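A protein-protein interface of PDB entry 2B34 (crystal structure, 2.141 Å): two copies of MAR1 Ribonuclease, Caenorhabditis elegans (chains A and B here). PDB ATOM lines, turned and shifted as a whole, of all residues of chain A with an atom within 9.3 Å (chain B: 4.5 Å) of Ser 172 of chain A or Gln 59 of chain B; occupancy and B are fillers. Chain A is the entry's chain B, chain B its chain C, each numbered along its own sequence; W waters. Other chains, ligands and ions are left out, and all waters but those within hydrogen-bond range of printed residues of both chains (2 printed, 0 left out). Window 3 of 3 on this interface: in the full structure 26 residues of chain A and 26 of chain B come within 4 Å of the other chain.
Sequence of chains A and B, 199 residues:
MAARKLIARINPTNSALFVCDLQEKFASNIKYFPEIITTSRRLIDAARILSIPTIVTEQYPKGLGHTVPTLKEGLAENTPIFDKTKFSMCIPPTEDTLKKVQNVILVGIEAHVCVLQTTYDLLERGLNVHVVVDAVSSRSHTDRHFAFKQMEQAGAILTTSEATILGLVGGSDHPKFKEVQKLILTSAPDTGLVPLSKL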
ATOM      1  N   LEU A 166       3.072   2.816 -24.237  1.00  0.00           N
ATOM      2  CA  LEU A 166       3.983   3.937 -24.447  1.00  0.00           C
ATOM      3  C   LEU A 166       5.387   3.660 -23.931  1.00  0.00           C
ATOM      4  O   LEU A 166       6.362   4.163 -24.489  1.00  0.00           O
ATOM      5  CB  LEU A 166       3.429   5.236 -23.851  1.00  0.00           C
ATOM      6  CG  LEU A 166       2.287   5.880 -24.643  1.00  0.00           C
ATOM      7  CD1 LEU A 166       1.679   7.051 -23.896  1.00  0.00           C
ATOM      8  CD2 LEU A 166       2.746   6.311 -26.028  1.00  0.00           C
ATOM      9  N   VAL A 169       7.716   2.056 -26.601  1.00  0.00           N
ATOM     10  CA  VAL A 169       8.265   2.881 -27.682  1.00  0.00           C
ATOM     11  C   VAL A 169       9.197   4.002 -27.201  1.00  0.00           C
ATOM     12  O   VAL A 169      10.093   4.412 -27.933  1.00  0.00           O
ATOM     13  CB  VAL A 169       7.164   3.432 -28.640  1.00  0.00           C
ATOM     14  CG1 VAL A 169       6.526   2.294 -29.427  1.00  0.00           C
ATOM     15  CG2 VAL A 169       6.112   4.250 -27.880  1.00  0.00           C
ATOM     16  N   GLY A 170       8.966   4.508 -25.989  1.00  0.00           N
ATOM     17  CA  GLY A 170       9.917   5.397 -25.319  1.00  0.00           C
ATOM     18  C   GLY A 170       9.974   6.850 -25.759  1.00  0.00           C
ATOM     19  O   GLY A 170      10.590   7.673 -25.083  1.00  0.00           O
ATOM     20  N   GLY A 171       9.338   7.164 -26.885  1.00  0.00           N
ATOM     21  CA  GLY A 171       9.285   8.532 -27.392  1.00  0.00           C
ATOM     22  C   GLY A 171       8.436   8.661 -28.644  1.00  0.00           C
ATOM     23  O   GLY A 171       8.113   7.664 -29.291  1.00  0.00           O
ATOM     24  N   SER A 172       8.084   9.896 -28.988  1.00  0.00           N
ATOM     25  CA  SER A 172       7.218  10.159 -30.144  1.00  0.00           C
ATOM     26  C   SER A 172       7.953  10.114 -31.495  1.00  0.00           C
ATOM     27  O   SER A 172       7.319  10.181 -32.552  1.00  0.00           O
ATOM     28  CB  SER A 172       6.474  11.484 -29.966  1.00  0.00           C
ATOM     29  OG  SER A 172       7.385  12.535 -29.740  1.00  0.00           O
ATOM     30  N   ASP A 173       9.281  10.000 -31.456  1.00  0.00           N
ATOM     31  CA  ASP A 173      10.077   9.815 -32.674  1.00  0.00           C
ATOM     32  C   ASP A 173      10.173   8.355 -33.122  1.00  0.00           C
ATOM     33  O   ASP A 173      10.610   8.077 -34.244  1.00  0.00           O
ATOM     34  CB  ASP A 173      11.479  10.412 -32.519  1.00  0.00           C
ATOM     35  CG  ASP A 173      11.536  11.881 -32.898  1.00  0.00           C
ATOM     36  OD1 ASP A 173      10.522  12.431 -33.384  1.00  0.00           O
ATOM     37  OD2 ASP A 173      12.609  12.491 -32.710  1.00  0.00           O
ATOM     38  N   HIS A 174       9.767   7.432 -32.249  1.00  0.00           N
ATOM     39  CA  HIS A 174       9.776   6.005 -32.573  1.00  0.00           C
ATOM     40  C   HIS A 174       8.970   5.755 -33.855  1.00  0.00           C
ATOM     41  O   HIS A 174       7.887   6.318 -34.016  1.00  0.00           O
ATOM     42  CB  HIS A 174       9.216   5.180 -31.408  1.00  0.00           C
ATOM     43  CG  HIS A 174       9.549   3.720 -31.486  1.00  0.00           C
ATOM     44  ND1 HIS A 174       8.849   2.838 -32.280  1.00  0.00           N
ATOM     45  CD2 HIS A 174      10.511   2.989 -30.872  1.00  0.00           C
ATOM     46  CE1 HIS A 174       9.363   1.628 -32.155  1.00  0.00           C
ATOM     47  NE2 HIS A 174      10.372   1.691 -31.303  1.00  0.00           N
ATOM     48  N   PRO A 175       9.508   4.932 -34.781  1.00  0.00           N
ATOM     49  CA  PRO A 175       8.832   4.646 -36.051  1.00  0.00           C
ATOM     50  C   PRO A 175       7.405   4.117 -35.893  1.00  0.00           C
ATOM     51  O   PRO A 175       6.552   4.401 -36.733  1.00  0.00           O
ATOM     52  CB  PRO A 175       9.723   3.576 -36.700  1.00  0.00           C
ATOM     53  CG  PRO A 175      10.582   3.063 -35.616  1.00  0.00           C
ATOM     54  CD  PRO A 175      10.798   4.229 -34.702  1.00  0.00           C
ATOM     55  N   LYS A 176       7.154   3.375 -34.818  1.00  0.00           N
ATOM     56  CA  LYS A 176       5.831   2.819 -34.554  1.00  0.00           C
ATOM     57  C   LYS A 176       4.956   3.676 -33.632  1.00  0.00           C
ATOM     58  O   LYS A 176       3.821   3.295 -33.338  1.00  0.00           O
ATOM     59  CB  LYS A 176       5.952   1.395 -33.997  1.00  0.00           C
ATOM     60  CG  LYS A 176       6.454   0.348 -35.002  1.00  0.00           C
ATOM     61  CD  LYS A 176       5.573   0.286 -36.251  1.00  0.00           C
ATOM     62  CE  LYS A 176       5.785  -1.000 -37.036  1.00  0.00           C
ATOM     63  NZ  LYS A 176       7.214  -1.259 -37.353  1.00  0.00           N
ATOM     64  N   PHE A 177       5.466   4.826 -33.186  1.00  0.00           N
ATOM     65  CA  PHE A 177       4.732   5.644 -32.211  1.00  0.00           C
ATOM     66  C   PHE A 177       3.288   5.940 -32.613  1.00  0.00           C
ATOM     67  O   PHE A 177       2.363   5.663 -31.851  1.00  0.00           O
ATOM     68  CB  PHE A 177       5.451   6.956 -31.881  1.00  0.00           C
ATOM     69  CG  PHE A 177       4.595   7.928 -31.100  1.00  0.00           C
ATOM     70  CD1 PHE A 177       4.298   7.695 -29.758  1.00  0.00           C
ATOM     71  CD2 PHE A 177       4.067   9.063 -31.714  1.00  0.00           C
ATOM     72  CE1 PHE A 177       3.501   8.579 -29.032  1.00  0.00           C
ATOM     73  CE2 PHE A 177       3.270   9.959 -30.998  1.00  0.00           C
ATOM     74  CZ  PHE A 177       2.988   9.715 -29.652  1.00  0.00           C
ATOM     75  N   LYS A 178       3.102   6.508 -33.803  1.00  0.00           N
ATOM     76  CA  LYS A 178       1.771   6.929 -34.244  1.00  0.00           C
ATOM     77  C   LYS A 178       0.806   5.747 -34.367  1.00  0.00           C
ATOM     78  O   LYS A 178      -0.393   5.892 -34.121  1.00  0.00           O
ATOM     79  CB  LYS A 178       1.845   7.713 -35.561  1.00  0.00           C
ATOM     80  CG  LYS A 178       2.667   9.010 -35.502  1.00  0.00           C
ATOM     81  CD  LYS A 178       2.031  10.080 -34.606  1.00  0.00           C
ATOM     82  CE  LYS A 178       2.893  11.342 -34.563  1.00  0.00           C
ATOM     83  NZ  LYS A 178       2.362  12.372 -33.607  1.00  0.00           N
ATOM     84  N   GLU A 179       1.343   4.585 -34.736  1.00  0.00           N
ATOM     85  CA  GLU A 179       0.555   3.357 -34.889  1.00  0.00           C
ATOM     86  C   GLU A 179       0.027   2.828 -33.550  1.00  0.00           C
ATOM     87  O   GLU A 179      -1.137   2.442 -33.451  1.00  0.00           O
ATOM     88  CB  GLU A 179       1.379   2.281 -35.602  1.00  0.00           C
ATOM     89  CG  GLU A 179       0.543   1.262 -36.356  1.00  0.00           C
ATOM     90  CD  GLU A 179       1.361   0.386 -37.293  1.00  0.00           C
ATOM     91  OE1 GLU A 179       2.417   0.841 -37.781  1.00  0.00           O
ATOM     92  OE2 GLU A 179       0.932  -0.762 -37.548  1.00  0.00           O
ATOM     93  N   VAL A 180       0.874   2.821 -32.522  1.00  0.00           N
ATOM     94  CA  VAL A 180       0.436   2.393 -31.185  1.00  0.00           C
ATOM     95  C   VAL A 180      -0.320   3.493 -30.433  1.00  0.00           C
ATOM     96  O   VAL A 180      -1.133   3.199 -29.556  1.00  0.00           O
ATOM     97  CB  VAL A 180       1.592   1.799 -30.313  1.00  0.00           C
ATOM     98  CG1 VAL A 180       2.293   0.656 -31.044  1.00  0.00           C
ATOM     99  CG2 VAL A 180       2.592   2.872 -29.884  1.00  0.00           C
ATOM    100  N   GLN A 181      -0.060   4.754 -30.792  1.00  0.00           N
ATOM    101  CA  GLN A 181      -0.771   5.895 -30.206  1.00  0.00           C
ATOM    102  C   GLN A 181      -2.267   5.796 -30.485  1.00  0.00           C
ATOM    103  O   GLN A 181      -3.086   6.148 -29.630  1.00  0.00           O
ATOM    104  CB  GLN A 181      -0.223   7.227 -30.730  1.00  0.00           C
ATOM    105  CG  GLN A 181      -0.845   8.469 -30.075  1.00  0.00           C
ATOM    106  CD  GLN A 181      -0.610   9.745 -30.866  1.00  0.00           C
ATOM    107  OE1 GLN A 181      -0.721   9.762 -32.091  1.00  0.00           O
ATOM    108  NE2 GLN A 181      -0.286  10.824 -30.164  1.00  0.00           N
ATOM    109  N   ASP B  21       7.010  18.597 -18.405  1.00  0.00           N
ATOM    110  CA  ASP B  21       6.025  18.741 -19.487  1.00  0.00           C
ATOM    111  C   ASP B  21       4.659  19.304 -19.085  1.00  0.00           C
ATOM    112  O   ASP B  21       3.624  18.886 -19.612  1.00  0.00           O
ATOM    113  CB  ASP B  21       5.855  17.397 -20.217  1.00  0.00           C
ATOM    114  CG  ASP B  21       7.166  16.856 -20.762  1.00  0.00           C
ATOM    115  OD1 ASP B  21       8.171  17.603 -20.788  1.00  0.00           O
ATOM    116  OD2 ASP B  21       7.193  15.679 -21.172  1.00  0.00           O
ATOM    117  N   GLN B  23       2.426  21.561 -19.805  1.00  0.00           N
ATOM    118  CA  GLN B  23       2.101  22.438 -20.926  1.00  0.00           C
ATOM    119  C   GLN B  23       0.610  22.722 -21.063  1.00  0.00           C
ATOM    120  O   GLN B  23      -0.226  21.958 -20.572  1.00  0.00           O
ATOM    121  CB  GLN B  23       2.650  21.857 -22.227  1.00  0.00           C
ATOM    122  CG  GLN B  23       4.163  21.847 -22.278  1.00  0.00           C
ATOM    123  CD  GLN B  23       4.696  20.743 -23.153  1.00  0.00           C
ATOM    124  OE1 GLN B  23       4.744  20.867 -24.374  1.00  0.00           O
ATOM    125  NE2 GLN B  23       5.101  19.649 -22.531  1.00  0.00           N
ATOM    126  N   THR B  57      11.315  20.677 -18.907  1.00  0.00           N
ATOM    127  CA  THR B  57      11.194  20.148 -20.263  1.00  0.00           C
ATOM    128  C   THR B  57       9.803  20.386 -20.841  1.00  0.00           C
ATOM    129  O   THR B  57       8.832  20.588 -20.109  1.00  0.00           O
ATOM    130  CB  THR B  57      11.549  18.641 -20.361  1.00  0.00           C
ATOM    131  OG1 THR B  57      10.695  17.885 -19.496  1.00  0.00           O
ATOM    132  CG2 THR B  57      13.009  18.392 -19.989  1.00  0.00           C
ATOM    133  N   GLU B  58       9.730  20.372 -22.165  1.00  0.00           N
ATOM    134  CA  GLU B  58       8.467  20.420 -22.880  1.00  0.00           C
ATOM    135  C   GLU B  58       8.497  19.356 -23.972  1.00  0.00           C
ATOM    136  O   GLU B  58       9.510  19.183 -24.652  1.00  0.00           O
ATOM    137  CB  GLU B  58       8.236  21.808 -23.484  1.00  0.00           C
ATOM    138  CG  GLU B  58       8.145  22.944 -22.459  1.00  0.00           C
ATOM    139  CD  GLU B  58       8.064  24.325 -23.095  1.00  0.00           C
ATOM    140  OE1 GLU B  58       8.191  24.434 -24.330  1.00  0.00           O
ATOM    141  OE2 GLU B  58       7.880  25.308 -22.352  1.00  0.00           O
ATOM    142  N   GLN B  59       7.394  18.628 -24.101  1.00  0.00           N
ATOM    143  CA  GLN B  59       7.215  17.631 -25.148  1.00  0.00           C
ATOM    144  C   GLN B  59       6.467  18.296 -26.306  1.00  0.00           C
ATOM    145  O   GLN B  59       5.424  18.900 -26.088  1.00  0.00           O
ATOM    146  CB  GLN B  59       6.411  16.449 -24.587  1.00  0.00           C
ATOM    147  CG  GLN B  59       6.079  15.332 -25.583  1.00  0.00           C
ATOM    148  CD  GLN B  59       7.120  14.222 -25.631  1.00  0.00           C
ATOM    149  OE1 GLN B  59       7.083  13.370 -26.519  1.00  0.00           O
ATOM    150  NE2 GLN B  59       8.046  14.221 -24.681  1.00  0.00           N
ATOM    151  N   TYR B  60       7.000  18.202 -27.524  1.00  0.00           N
ATOM    152  CA  TYR B  60       6.351  18.785 -28.715  1.00  0.00           C
ATOM    153  C   TYR B  60       5.629  20.115 -28.448  1.00  0.00           C
ATOM    154  O   TYR B  60       4.407  20.184 -28.596  1.00  0.00           O
ATOM    155  CB  TYR B  60       5.340  17.793 -29.310  1.00  0.00           C
ATOM    156  CG  TYR B  60       5.865  16.937 -30.434  1.00  0.00           C
ATOM    157  CD1 TYR B  60       6.905  16.031 -30.221  1.00  0.00           C
ATOM    158  CD2 TYR B  60       5.306  17.013 -31.710  1.00  0.00           C
ATOM    159  CE1 TYR B  60       7.389  15.236 -31.257  1.00  0.00           C
ATOM    160  CE2 TYR B  60       5.785  16.216 -32.757  1.00  0.00           C
ATOM    161  CZ  TYR B  60       6.826  15.330 -32.518  1.00  0.00           C
ATOM    162  OH  TYR B  60       7.312  14.536 -33.531  1.00  0.00           O
ATOM    163  N   PRO B  61       6.373  21.173 -28.058  1.00  0.00           N
ATOM    164  CA  PRO B  61       5.739  22.444 -27.674  1.00  0.00           C
ATOM    165  C   PRO B  61       4.876  23.092 -28.765  1.00  0.00           C
ATOM    166  O   PRO B  61       3.986  23.885 -28.443  1.00  0.00           O
ATOM    167  CB  PRO B  61       6.930  23.349 -27.338  1.00  0.00           C
ATOM    168  CG  PRO B  61       8.053  22.427 -27.073  1.00  0.00           C
ATOM    169  CD  PRO B  61       7.840  21.240 -27.944  1.00  0.00           C
ATOM    170  N   LEU B  64       1.697  20.756 -28.263  1.00  0.00           N
ATOM    171  CA  LEU B  64       1.243  20.634 -26.880  1.00  0.00           C
ATOM    172  C   LEU B  64       1.296  21.945 -26.094  1.00  0.00           C
ATOM    173  O   LEU B  64       0.881  21.998 -24.933  1.00  0.00           O
ATOM    174  CB  LEU B  64       2.029  19.521 -26.169  1.00  0.00           C
ATOM    175  CG  LEU B  64       1.888  18.123 -26.798  1.00  0.00           C
ATOM    176  CD1 LEU B  64       2.813  17.106 -26.148  1.00  0.00           C
ATOM    177  CD2 LEU B  64       0.439  17.638 -26.754  1.00  0.00           C
ATOM    178  N   LYS B  84      11.752  18.184 -26.067  1.00  0.00           N
ATOM    179  CA  LYS B  84      12.099  16.780 -26.263  1.00  0.00           C
ATOM    180  C   LYS B  84      10.974  16.031 -26.965  1.00  0.00           C
ATOM    181  O   LYS B  84       9.839  16.508 -27.019  1.00  0.00           O
ATOM    182  CB  LYS B  84      12.438  16.102 -24.922  1.00  0.00           C
ATOM    183  CG  LYS B  84      11.291  16.072 -23.904  1.00  0.00           C
ATOM    184  CD  LYS B  84      11.715  15.392 -22.608  1.00  0.00           C
ATOM    185  CE  LYS B  84      10.550  15.257 -21.626  1.00  0.00           C
ATOM    186  NZ  LYS B  84       9.495  14.320 -22.115  1.00  0.00           N
ATOM    187  N   THR B  85      11.312  14.867 -27.513  1.00  0.00           N
ATOM    188  CA  THR B  85      10.329  13.929 -28.053  1.00  0.00           C
ATOM    189  C   THR B  85      10.393  12.633 -27.249  1.00  0.00           C
ATOM    190  O   THR B  85       9.418  11.886 -27.179  1.00  0.00           O
ATOM    191  CB  THR B  85      10.570  13.629 -29.551  1.00  0.00           C
ATOM    192  OG1 THR B  85      11.786  12.889 -29.704  1.00  0.00           O
ATOM    193  CG2 THR B  85      10.661  14.919 -30.351  1.00  0.00           C
ATOM    194  N   LYS B  86      11.553  12.378 -26.650  1.00  0.00           N
ATOM    195  CA  LYS B  86      11.737  11.268 -25.724  1.00  0.00           C
ATOM    196  C   LYS B  86      10.874  11.507 -24.488  1.00  0.00           C
ATOM    197  O   LYS B  86      10.746  12.639 -24.029  1.00  0.00           O
ATOM    198  CB  LYS B  86      13.212  11.157 -25.335  1.00  0.00           C
ATOM    199  CG  LYS B  86      13.585   9.873 -24.616  1.00  0.00           C
ATOM    200  CD  LYS B  86      15.000   9.448 -24.978  1.00  0.00           C
ATOM    201  CE  LYS B  86      15.409   8.176 -24.249  1.00  0.00           C
ATOM    202  NZ  LYS B  86      16.502   7.457 -24.974  1.00  0.00           N
ATOM    203  N   PHE B  87      10.260  10.449 -23.966  1.00  0.00           N
ATOM    204  CA  PHE B  87       9.401  10.601 -22.795  1.00  0.00           C
ATOM    205  C   PHE B  87      10.203  11.018 -21.555  1.00  0.00           C
ATOM    206  O   PHE B  87       9.803  11.926 -20.817  1.00  0.00           O
ATOM    207  CB  PHE B  87       8.542   9.350 -22.562  1.00  0.00           C
ATOM    208  CG  PHE B  87       7.618   9.020 -23.719  1.00  0.00           C
ATOM    209  CD1 PHE B  87       7.041  10.033 -24.490  1.00  0.00           C
ATOM    210  CD2 PHE B  87       7.313   7.697 -24.025  1.00  0.00           C
ATOM    211  CE1 PHE B  87       6.194   9.732 -25.556  1.00  0.00           C
ATOM    212  CE2 PHE B  87       6.464   7.386 -25.088  1.00  0.00           C
ATOM    213  CZ  PHE B  87       5.903   8.405 -25.854  1.00  0.00           C
ATOM    214  N   CYS B 114       6.096  10.092 -19.075  1.00  0.00           N
ATOM    215  CA  CYS B 114       7.310  10.907 -18.963  1.00  0.00           C
ATOM    216  C   CYS B 114       7.880  10.937 -17.539  1.00  0.00           C
ATOM    217  O   CYS B 114       9.091  10.806 -17.357  1.00  0.00           O
ATOM    218  CB  CYS B 114       7.079  12.324 -19.500  1.00  0.00           C
ATOM    219  SG  CYS B 114       6.797  12.416 -21.314  1.00  0.00           S
HETATM  220  O   HOH W   1      11.682   7.779 -22.493  1.00  0.00           O
HETATM  221  O   HOH W   2      11.461   9.950 -29.389  1.00  0.00           O
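The backbone carbonyl oxygen (O) of Gly 170 of chain A sits at hydrogen-bond distance from the backbone NH (N) of Phe 87 of chain B (3.0 Å). OE1 of Gln 59 of chain B lies within hydrogen-bond range of OG of Ser 172 of chain A. O of Thr 85 of chain B lies within hydrogen-bond range of N of Ser 172 of chain A (3.0 Å). OD2 of Asp 173 of chain A lies within hydrogen-bond range of OG1 of Thr 85 of chain B, 3.1 Å away.
Ser 172 of chain A touches just these residues of chain B: Gln 59, Tyr 60, Thr 85 and Phe 87. Of chain A, only Ser 172 comes within 4 Å of Gln 59 of chain B. No residue of chain A comes within 4 Å of Lys 84 of chain B. Printed residues of chain A within 4 Å of Thr 85 of chain B: Gly 171, Ser 172 and Asp 173. Of the printed residues of chain B, Leu 166 of chain A touches Phe 87. Printed residues of chain B within 4 Å of Gly 170 of chain A: Lys 86 and Phe 87. Of the printed residues of chain B, Gly 171 of chain A touches Thr 85 and Phe 87. Leu 64 of chain B touches none of the printed residues of chain A. The nearest printed residue of chain B that does not touch Ser 172 of chain A is Lys 86 of chain B (4.9 Å). The nearest residue of chain A that does not touch Gln 59 of chain B is Gly 171 of chain A (5.3 Å). The nearest printed residue of chain A that does not touch Tyr 60 of chain B is Lys 178 of chain A (5.2 Å).
No position is printed for both chains. Of the 12 pairs that touch across the chains among the printed residues, none has its exchanged pair printed and touching as well.
OE1 of Gln 23 of chain B sits close to O of Gln 59 of chain B (2.7 Å). The side-chain amide nitrogen (NE2) of Gln 59 of chain B lies close to the side-chain amino group (NZ) of Lys 84 of chain B, 2.9 Å away. O of Thr 85 of chain B lies close to OE1 of Gln 59 of chain B, at 2.8 Å. N of Tyr 60 of chain B sits at hydrogen-bond distance from O of Lys 84 of chain B, at 3.3 Å. O of Lys 86 of chain B lies within hydrogen-bond range of NZ of Lys 84 of chain B, 2.8 Å away. The backbone carbonyl oxygen (O) of Phe 87 of chain B lies close to the side-chain sulfur (SG) of Cys 114 of chain B (3.1 Å).
Of the 13 printed residues of chain B, 5 touch a printed residue of chain A. Among the printed residues, 12 pairs touch across the chains.
Among the printed residues, pairs that only touch across the chains: Leu 166 of chain A with Phe 87 of chain B (3.3 Å), Gly 170 of chain A with Lys 86 of chain B (3.7 Å), Gly 171 of chain A with Thr 85 of chain B (3.4 Å), Gly 171 of chain A with Phe 87 of chain B (3.4 Å), Ser 172 of chain A with Tyr 60 of chain B (3.1 Å), Ser 172 of chain A with Phe 87 of chain B (3.9 Å), Asp 173 of chain A with Tyr 60 of chain B (3.8 Å) and Phe 177 of chain A with Phe 87 of chain B (3.99 Å).
Water W1 bridges the backbone carbonyl oxygen of Gly 170 of chain A and the backbone NH of Phe 87 of chain B. Water W2 lies within hydrogen-bond range of OG1 of Thr 85 of chain B (3.0 Å), N of Asp 173 of chain A (3.0 Å) and N of Ser 172 of chain A (3.4 Å).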
